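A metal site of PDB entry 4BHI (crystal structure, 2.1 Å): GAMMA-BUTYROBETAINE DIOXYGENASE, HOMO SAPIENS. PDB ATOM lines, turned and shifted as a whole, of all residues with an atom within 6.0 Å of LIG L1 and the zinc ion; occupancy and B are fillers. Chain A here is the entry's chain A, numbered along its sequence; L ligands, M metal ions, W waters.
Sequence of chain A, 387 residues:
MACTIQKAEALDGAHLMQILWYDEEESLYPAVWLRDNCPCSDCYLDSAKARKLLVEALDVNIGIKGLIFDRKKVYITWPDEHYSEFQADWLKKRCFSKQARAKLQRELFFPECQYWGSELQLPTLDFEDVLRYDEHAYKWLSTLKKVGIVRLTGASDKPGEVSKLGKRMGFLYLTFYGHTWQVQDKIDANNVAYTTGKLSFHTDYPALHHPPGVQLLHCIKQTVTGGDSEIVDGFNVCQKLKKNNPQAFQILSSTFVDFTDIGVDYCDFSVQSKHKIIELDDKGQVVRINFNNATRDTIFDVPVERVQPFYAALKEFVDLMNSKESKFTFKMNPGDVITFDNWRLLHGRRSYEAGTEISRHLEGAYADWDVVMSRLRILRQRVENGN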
ATOM      1  N   TRP A 181     -39.393 -12.326 -15.241  1.00  0.00           N
ATOM      2  CA  TRP A 181     -38.393 -12.551 -14.201  1.00  0.00           C
ATOM      3  C   TRP A 181     -37.911 -11.200 -13.694  1.00  0.00           C
ATOM      4  O   TRP A 181     -37.973 -10.192 -14.412  1.00  0.00           O
ATOM      5  CB  TRP A 181     -37.199 -13.402 -14.719  1.00  0.00           C
ATOM      6  CG  TRP A 181     -36.941 -13.286 -16.196  1.00  0.00           C
ATOM      7  CD1 TRP A 181     -37.441 -14.097 -17.157  1.00  0.00           C
ATOM      8  CD2 TRP A 181     -36.137 -12.317 -16.862  1.00  0.00           C
ATOM      9  NE1 TRP A 181     -37.027 -13.687 -18.395  1.00  0.00           N
ATOM     10  CE2 TRP A 181     -36.229 -12.593 -18.243  1.00  0.00           C
ATOM     11  CE3 TRP A 181     -35.359 -11.255 -16.441  1.00  0.00           C
ATOM     12  CZ2 TRP A 181     -35.554 -11.847 -19.194  1.00  0.00           C
ATOM     13  CZ3 TRP A 181     -34.706 -10.505 -17.391  1.00  0.00           C
ATOM     14  CH2 TRP A 181     -34.790 -10.820 -18.750  1.00  0.00           C
ATOM     15  N   VAL A 183     -34.972  -8.900 -12.241  1.00  0.00           N
ATOM     16  CA  VAL A 183     -33.543  -8.673 -12.165  1.00  0.00           C
ATOM     17  C   VAL A 183     -33.285  -7.808 -10.950  1.00  0.00           C
ATOM     18  O   VAL A 183     -33.561  -6.613 -10.952  1.00  0.00           O
ATOM     19  CB  VAL A 183     -32.981  -8.004 -13.433  1.00  0.00           C
ATOM     20  CG1 VAL A 183     -31.485  -7.827 -13.327  1.00  0.00           C
ATOM     21  CG2 VAL A 183     -33.315  -8.836 -14.643  1.00  0.00           C
ATOM     22  N   ASN A 191     -28.153 -17.078 -10.615  1.00  0.00           N
ATOM     23  CA  ASN A 191     -27.693 -16.483 -11.868  1.00  0.00           C
ATOM     24  C   ASN A 191     -26.932 -15.209 -11.544  1.00  0.00           C
ATOM     25  O   ASN A 191     -27.368 -14.421 -10.694  1.00  0.00           O
ATOM     26  CB  ASN A 191     -28.903 -16.185 -12.798  1.00  0.00           C
ATOM     27  CG  ASN A 191     -28.493 -15.972 -14.258  1.00  0.00           C
ATOM     28  OD1 ASN A 191     -28.044 -14.891 -14.637  1.00  0.00           O
ATOM     29  ND2 ASN A 191     -28.689 -16.985 -15.085  1.00  0.00           N
ATOM     30  N   ALA A 193     -26.898 -12.628 -13.125  1.00  0.00           N
ATOM     31  CA  ALA A 193     -27.825 -11.502 -13.351  1.00  0.00           C
ATOM     32  C   ALA A 193     -28.447 -10.992 -12.035  1.00  0.00           C
ATOM     33  O   ALA A 193     -28.656  -9.791 -11.859  1.00  0.00           O
ATOM     34  CB  ALA A 193     -28.909 -11.883 -14.342  1.00  0.00           C
ATOM     35  N   TYR A 194     -28.697 -11.918 -11.097  1.00  0.00           N
ATOM     36  CA  TYR A 194     -29.387 -11.632  -9.830  1.00  0.00           C
ATOM     37  C   TYR A 194     -28.416 -11.289  -8.677  1.00  0.00           C
ATOM     38  O   TYR A 194     -28.581 -11.761  -7.528  1.00  0.00           O
ATOM     39  CB  TYR A 194     -30.285 -12.826  -9.448  1.00  0.00           C
ATOM     40  CG  TYR A 194     -31.321 -13.203 -10.519  1.00  0.00           C
ATOM     41  CD1 TYR A 194     -31.821 -12.247 -11.410  1.00  0.00           C
ATOM     42  CD2 TYR A 194     -31.783 -14.511 -10.640  1.00  0.00           C
ATOM     43  CE1 TYR A 194     -32.727 -12.573 -12.376  1.00  0.00           C
ATOM     44  CE2 TYR A 194     -32.706 -14.851 -11.630  1.00  0.00           C
ATOM     45  CZ  TYR A 194     -33.172 -13.867 -12.474  1.00  0.00           C
ATOM     46  OH  TYR A 194     -34.085 -14.119 -13.451  1.00  0.00           O
ATOM     47  N   LEU A 199     -22.139  -7.005 -15.529  1.00  0.00           N
ATOM     48  CA  LEU A 199     -22.343  -7.972 -16.592  1.00  0.00           C
ATOM     49  C   LEU A 199     -21.638  -7.419 -17.811  1.00  0.00           C
ATOM     50  O   LEU A 199     -22.002  -6.348 -18.320  1.00  0.00           O
ATOM     51  CB  LEU A 199     -23.844  -8.187 -16.884  1.00  0.00           C
ATOM     52  CG  LEU A 199     -24.707  -8.641 -15.692  1.00  0.00           C
ATOM     53  CD1 LEU A 199     -26.170  -8.737 -16.045  1.00  0.00           C
ATOM     54  CD2 LEU A 199     -24.252  -9.999 -15.194  1.00  0.00           C
ATOM     55  N   HIS A 202     -23.007  -9.674 -23.332  1.00  0.00           N
ATOM     56  CA  HIS A 202     -23.467 -11.013 -23.597  1.00  0.00           C
ATOM     57  C   HIS A 202     -24.808 -10.975 -24.312  1.00  0.00           C
ATOM     58  O   HIS A 202     -25.455  -9.932 -24.370  1.00  0.00           O
ATOM     59  CB  HIS A 202     -23.675 -11.724 -22.262  1.00  0.00           C
ATOM     60  CG  HIS A 202     -24.755 -11.128 -21.439  1.00  0.00           C
ATOM     61  ND1 HIS A 202     -24.563 -10.001 -20.679  1.00  0.00           N
ATOM     62  CD2 HIS A 202     -26.058 -11.453 -21.307  1.00  0.00           C
ATOM     63  CE1 HIS A 202     -25.708  -9.672 -20.095  1.00  0.00           C
ATOM     64  NE2 HIS A 202     -26.618 -10.556 -20.437  1.00  0.00           N
ATOM     65  N   THR A 203     -25.202 -12.126 -24.845  1.00  0.00           N
ATOM     66  CA  THR A 203     -26.567 -12.399 -25.241  1.00  0.00           C
ATOM     67  C   THR A 203     -27.168 -13.268 -24.151  1.00  0.00           C
ATOM     68  O   THR A 203     -26.443 -13.989 -23.473  1.00  0.00           O
ATOM     69  CB  THR A 203     -26.611 -13.162 -26.580  1.00  0.00           C
ATOM     70  OG1 THR A 203     -25.855 -14.390 -26.485  1.00  0.00           O
ATOM     71  CG2 THR A 203     -26.004 -12.310 -27.694  1.00  0.00           C
ATOM     72  N   ASP A 204     -28.492 -13.205 -23.982  1.00  0.00           N
ATOM     73  CA  ASP A 204     -29.200 -14.053 -23.018  1.00  0.00           C
ATOM     74  C   ASP A 204     -29.466 -15.429 -23.565  1.00  0.00           C
ATOM     75  O   ASP A 204     -29.840 -15.602 -24.709  1.00  0.00           O
ATOM     76  CB  ASP A 204     -30.541 -13.447 -22.595  1.00  0.00           C
ATOM     77  CG  ASP A 204     -30.420 -12.482 -21.452  1.00  0.00           C
ATOM     78  OD1 ASP A 204     -29.361 -11.825 -21.332  1.00  0.00           O
ATOM     79  OD2 ASP A 204     -31.402 -12.382 -20.675  1.00  0.00           O
ATOM     80  N   GLN A 215     -35.772  -9.485 -26.408  1.00  0.00           N
ATOM     81  CA  GLN A 215     -35.792  -9.308 -24.969  1.00  0.00           C
ATOM     82  C   GLN A 215     -36.500  -8.013 -24.637  1.00  0.00           C
ATOM     83  O   GLN A 215     -36.369  -7.019 -25.340  1.00  0.00           O
ATOM     84  CB  GLN A 215     -34.366  -9.275 -24.406  1.00  0.00           C
ATOM     85  CG  GLN A 215     -34.314  -9.274 -22.878  1.00  0.00           C
ATOM     86  CD  GLN A 215     -32.917  -9.320 -22.298  1.00  0.00           C
ATOM     87  OE1 GLN A 215     -32.662  -8.709 -21.272  1.00  0.00           O
ATOM     88  NE2 GLN A 215     -32.005 -10.058 -22.938  1.00  0.00           N
ATOM     89  N   LEU A 217     -37.058  -5.423 -21.271  1.00  0.00           N
ATOM     90  CA  LEU A 217     -36.509  -5.105 -19.955  1.00  0.00           C
ATOM     91  C   LEU A 217     -37.067  -3.797 -19.470  1.00  0.00           C
ATOM     92  O   LEU A 217     -36.872  -2.766 -20.094  1.00  0.00           O
ATOM     93  CB  LEU A 217     -34.981  -4.975 -19.989  1.00  0.00           C
ATOM     94  CG  LEU A 217     -34.066  -6.109 -19.514  1.00  0.00           C
ATOM     95  CD1 LEU A 217     -32.641  -5.574 -19.394  1.00  0.00           C
ATOM     96  CD2 LEU A 217     -34.513  -6.660 -18.193  1.00  0.00           C
ATOM     97  N   GLY A 227     -25.101   0.659 -12.321  1.00  0.00           N
ATOM     98  CA  GLY A 227     -26.227   0.040 -13.028  1.00  0.00           C
ATOM     99  C   GLY A 227     -26.581   0.608 -14.387  1.00  0.00           C
ATOM    100  O   GLY A 227     -27.666   0.341 -14.897  1.00  0.00           O
ATOM    101  N   ASP A 228     -25.651   1.354 -15.006  1.00  0.00           N
ATOM    102  CA  ASP A 228     -25.855   1.845 -16.360  1.00  0.00           C
ATOM    103  C   ASP A 228     -25.929   0.646 -17.285  1.00  0.00           C
ATOM    104  O   ASP A 228     -25.375  -0.403 -16.967  1.00  0.00           O
ATOM    105  CB  ASP A 228     -24.708   2.750 -16.855  1.00  0.00           C
ATOM    106  CG  ASP A 228     -24.456   3.934 -15.954  1.00  0.00           C
ATOM    107  OD1 ASP A 228     -23.895   3.726 -14.869  1.00  0.00           O
ATOM    108  OD2 ASP A 228     -24.793   5.063 -16.349  1.00  0.00           O
ATOM    109  N   SER A 229     -26.604   0.835 -18.415  1.00  0.00           N
ATOM    110  CA  SER A 229     -26.727  -0.175 -19.454  1.00  0.00           C
ATOM    111  C   SER A 229     -25.737   0.143 -20.574  1.00  0.00           C
ATOM    112  O   SER A 229     -25.381   1.316 -20.822  1.00  0.00           O
ATOM    113  CB  SER A 229     -28.150  -0.189 -20.004  1.00  0.00           C
ATOM    114  OG  SER A 229     -29.134  -0.323 -18.975  1.00  0.00           O
ATOM    115  N   ASN A 292     -22.617 -15.836 -23.679  1.00  0.00           N
ATOM    116  CA  ASN A 292     -22.668 -15.345 -22.316  1.00  0.00           C
ATOM    117  C   ASN A 292     -21.502 -15.993 -21.560  1.00  0.00           C
ATOM    118  O   ASN A 292     -21.351 -17.214 -21.558  1.00  0.00           O
ATOM    119  CB  ASN A 292     -24.015 -15.659 -21.679  1.00  0.00           C
ATOM    120  CG  ASN A 292     -24.194 -15.001 -20.305  1.00  0.00           C
ATOM    121  OD1 ASN A 292     -23.226 -14.725 -19.589  1.00  0.00           O
ATOM    122  ND2 ASN A 292     -25.438 -14.751 -19.928  1.00  0.00           N
ATOM    123  N   MET A 332     -31.148   3.469 -17.657  1.00  0.00           N
ATOM    124  CA  MET A 332     -32.596   3.376 -17.604  1.00  0.00           C
ATOM    125  C   MET A 332     -33.129   4.035 -16.326  1.00  0.00           C
ATOM    126  O   MET A 332     -32.519   3.942 -15.267  1.00  0.00           O
ATOM    127  CB  MET A 332     -33.033   1.911 -17.626  1.00  0.00           C
ATOM    128  CG  MET A 332     -32.566   1.108 -18.840  1.00  0.00           C
ATOM    129  SD  MET A 332     -33.303  -0.565 -18.865  1.00  0.00           S
ATOM    130  CE  MET A 332     -35.014  -0.118 -19.161  1.00  0.00           C
ATOM    131  N   HIS A 347     -25.510  -7.098 -24.695  1.00  0.00           N
ATOM    132  CA  HIS A 347     -25.858  -6.094 -23.726  1.00  0.00           C
ATOM    133  C   HIS A 347     -25.151  -6.381 -22.443  1.00  0.00           C
ATOM    134  O   HIS A 347     -24.631  -7.506 -22.229  1.00  0.00           O
ATOM    135  CB  HIS A 347     -27.365  -6.016 -23.546  1.00  0.00           C
ATOM    136  CG  HIS A 347     -27.981  -7.263 -22.976  1.00  0.00           C
ATOM    137  ND1 HIS A 347     -28.113  -8.425 -23.719  1.00  0.00           N
ATOM    138  CD2 HIS A 347     -28.452  -7.540 -21.746  1.00  0.00           C
ATOM    139  CE1 HIS A 347     -28.668  -9.359 -22.964  1.00  0.00           C
ATOM    140  NE2 HIS A 347     -28.886  -8.842 -21.764  1.00  0.00           N
ATOM    141  N   GLY A 348     -25.066  -5.351 -21.611  1.00  0.00           N
ATOM    142  CA  GLY A 348     -24.456  -5.480 -20.321  1.00  0.00           C
ATOM    143  C   GLY A 348     -24.869  -4.443 -19.320  1.00  0.00           C
ATOM    144  O   GLY A 348     -25.706  -3.569 -19.581  1.00  0.00           O
ATOM    145  N   ARG A 349     -24.245  -4.527 -18.168  1.00  0.00           N
ATOM    146  CA  ARG A 349     -24.645  -3.700 -17.045  1.00  0.00           C
ATOM    147  C   ARG A 349     -23.405  -3.369 -16.213  1.00  0.00           C
ATOM    148  O   ARG A 349     -22.564  -4.231 -15.992  1.00  0.00           O
ATOM    149  CB  ARG A 349     -25.652  -4.484 -16.201  1.00  0.00           C
ATOM    150  CG  ARG A 349     -25.740  -4.013 -14.769  1.00  0.00           C
ATOM    151  CD  ARG A 349     -26.687  -4.890 -13.974  1.00  0.00           C
ATOM    152  NE  ARG A 349     -26.010  -5.935 -13.256  1.00  0.00           N
ATOM    153  CZ  ARG A 349     -26.607  -7.031 -12.787  1.00  0.00           C
ATOM    154  NH1 ARG A 349     -27.906  -7.228 -12.993  1.00  0.00           N
ATOM    155  NH2 ARG A 349     -25.896  -7.928 -12.123  1.00  0.00           N
ATOM    156  N   ARG A 360     -32.577  -1.650  -6.792  1.00  0.00           N
ATOM    157  CA  ARG A 360     -32.595  -1.802  -8.240  1.00  0.00           C
ATOM    158  C   ARG A 360     -33.395  -3.018  -8.636  1.00  0.00           C
ATOM    159  O   ARG A 360     -33.174  -4.116  -8.106  1.00  0.00           O
ATOM    160  CB  ARG A 360     -31.169  -1.942  -8.774  1.00  0.00           C
ATOM    161  CG  ARG A 360     -31.076  -1.834 -10.291  1.00  0.00           C
ATOM    162  CD  ARG A 360     -29.652  -1.914 -10.758  1.00  0.00           C
ATOM    163  NE  ARG A 360     -29.509  -1.596 -12.187  1.00  0.00           N
ATOM    164  CZ  ARG A 360     -29.617  -2.463 -13.188  1.00  0.00           C
ATOM    165  NH1 ARG A 360     -29.934  -3.743 -12.987  1.00  0.00           N
ATOM    166  NH2 ARG A 360     -29.413  -2.036 -14.426  1.00  0.00           N
ATOM    167  N   LEU A 362     -35.401  -4.636 -12.216  1.00  0.00           N
ATOM    168  CA  LEU A 362     -35.910  -4.683 -13.574  1.00  0.00           C
ATOM    169  C   LEU A 362     -36.842  -5.896 -13.695  1.00  0.00           C
ATOM    170  O   LEU A 362     -36.649  -6.896 -13.000  1.00  0.00           O
ATOM    171  CB  LEU A 362     -34.760  -4.770 -14.587  1.00  0.00           C
ATOM    172  CG  LEU A 362     -33.548  -3.830 -14.553  1.00  0.00           C
ATOM    173  CD1 LEU A 362     -32.503  -4.264 -15.571  1.00  0.00           C
ATOM    174  CD2 LEU A 362     -33.899  -2.368 -14.802  1.00  0.00           C
ATOM    175  N   TYR A 366     -38.988 -12.605 -22.546  1.00  0.00           N
ATOM    176  CA  TYR A 366     -38.510 -12.927 -23.863  1.00  0.00           C
ATOM    177  C   TYR A 366     -39.669 -13.101 -24.836  1.00  0.00           C
ATOM    178  O   TYR A 366     -40.780 -13.435 -24.430  1.00  0.00           O
ATOM    179  CB  TYR A 366     -37.727 -14.235 -23.797  1.00  0.00           C
ATOM    180  CG  TYR A 366     -36.495 -14.206 -22.919  1.00  0.00           C
ATOM    181  CD1 TYR A 366     -35.477 -13.274 -23.135  1.00  0.00           C
ATOM    182  CD2 TYR A 366     -36.344 -15.116 -21.884  1.00  0.00           C
ATOM    183  CE1 TYR A 366     -34.340 -13.252 -22.341  1.00  0.00           C
ATOM    184  CE2 TYR A 366     -35.206 -15.116 -21.082  1.00  0.00           C
ATOM    185  CZ  TYR A 366     -34.196 -14.198 -21.331  1.00  0.00           C
ATOM    186  OH  TYR A 366     -33.060 -14.175 -20.537  1.00  0.00           O
HETATM  187  C1  LIG L   1     -29.504  -9.889 -17.481  1.00  0.00           C
HETATM  188  C2  LIG L   1     -29.150  -8.529 -17.915  1.00  0.00           C
HETATM  189  C3  LIG L   1     -29.290  -6.182 -17.450  1.00  0.00           C
HETATM  190  C4  LIG L   1     -29.299  -5.323 -16.218  1.00  0.00           C
HETATM  191  O1  LIG L   1     -29.099 -10.874 -18.154  1.00  0.00           O
HETATM  192  O2  LIG L   1     -30.207  -9.997 -16.429  1.00  0.00           O
HETATM  193  O3  LIG L   1     -28.510  -8.328 -18.956  1.00  0.00           O
HETATM  194  O4  LIG L   1     -29.217  -4.134 -16.472  1.00  0.00           O
HETATM  195  N1  LIG L   1     -29.569  -7.554 -17.129  1.00  0.00           N
HETATM  196  O5  LIG L   1     -29.392  -5.798 -15.067  1.00  0.00           O
HETATM  197  O1  LG2 L   2     -28.129 -16.302 -20.101  1.00  0.00           O
HETATM  198  C1  LG2 L   2     -28.298 -16.116 -18.884  1.00  0.00           C
HETATM  199  O2  LG2 L   2     -28.070 -17.028 -18.040  1.00  0.00           O
HETATM  200  C2  LG2 L   2     -28.712 -14.745 -18.347  1.00  0.00           C
HETATM  201  C3  LG2 L   2     -30.085 -14.234 -18.698  1.00  0.00           C
HETATM  202  N1  LG2 L   2     -31.147 -14.862 -17.896  1.00  0.00           N
HETATM  203  C4  LG2 L   2     -31.370 -16.241 -18.284  1.00  0.00           C
HETATM  204  N2  LG2 L   2     -31.907 -14.234 -16.921  1.00  0.00           N
HETATM  205  C5  LG2 L   2     -31.585 -14.748 -15.575  1.00  0.00           C
HETATM  206  C6  LG2 L   2     -31.741 -12.764 -16.912  1.00  0.00           C
HETATM  207  C7  LG2 L   2     -33.341 -14.476 -17.154  1.00  0.00           C
HETATM  208 ZN    ZN M   1     -28.725 -10.203 -20.079  1.00  0.00          ZN
HETATM  209  O   HOH W   1     -28.792  -3.045 -18.993  1.00  0.00           O
HETATM  210  O   HOH W   2     -26.446 -12.627 -17.391  1.00  0.00           O
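The guanidinium group of Arg 349 lies within salt-bridge range of an oxygen (O5) of LIG L1 (2.9 Å).
The guanidinium group of Arg 360 lies within salt-bridge range of an oxygen (O4) of LIG L1 (2.9 Å).
ND2 of Asn 191 sits at hydrogen-bond distance from O2 of LG2 L2 (3.0 Å).
ND2 of Asn 292 sits at hydrogen-bond distance from O1 of LG2 L2 (3.1 Å).
OH of Tyr 366 sits close to N1 of LG2 L2, 3.3 Å away.
The zinc ion is bound by an oxygen (O1) of LIG L1, at 2.1 Å.
OD1 of Asp 204 is bound to the zinc ion.
NE2 of His 202 binds the zinc ion, 2.2 Å away.
A ring nitrogen (NE2) of His 347 binds the zinc ion, 2.2 Å away.
The zinc ion is bound by O3 of LIG L1 (2.2 Å).
The zinc ion has five donor atoms within binding distance.
CG1 of Val 183 touches O5 of LIG L1, at 3.4 Å.
Ala 193 touches LIG L1.
Leu 199 touches LIG L1.
CD1 of Leu 217 touches C3 of LIG L1, 3.9 Å away.
Leu 362 touches LIG L1 (CD1 to O4, 3.4 Å).
Hydrophobic or aromatic side chains that line LIG L1: Val 183, Ala 193, Leu 199, His 202, Leu 217, His 347 and Leu 362.
The nearest printed residue that does not touch LIG L1 is Ser 229 (4.6 Å).
Water W1 lies within hydrogen-bond range of OG of Ser 229 (2.7 Å), O4 of LIG L1 (2.8 Å) and O of Gly 348 (3.2 Å).
The side-chain amide nitrogen (NE2) of Gln 215 lies close to the side-chain carboxylate (OD2) of Asp 204.
The side-chain carboxylate of Asp 204 is in hydrogen-bond range of the side-chain hydroxyl of Tyr 366 (2.4 Å).
NH1 of Arg 349 is in hydrogen-bond range of O of Ala 193.
The backbone carbonyl oxygen (O) of Arg 349 lies within hydrogen-bond range of the backbone NH (N) of Leu 199.
The backbone carbonyl oxygen of Gly 227 sits at hydrogen-bond distance from the guanidinium group of Arg 360 (3.0 Å).
The backbone NH of Ala 193 lies within hydrogen-bond range of the side-chain amide oxygen of Asn 191 (3.0 Å).
The backbone NH of Val 183 lies within hydrogen-bond range of the backbone carbonyl oxygen of Leu 362 (2.7 Å).
Within 4 Å of the zinc ion: His 202, Asp 204 and His 347.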
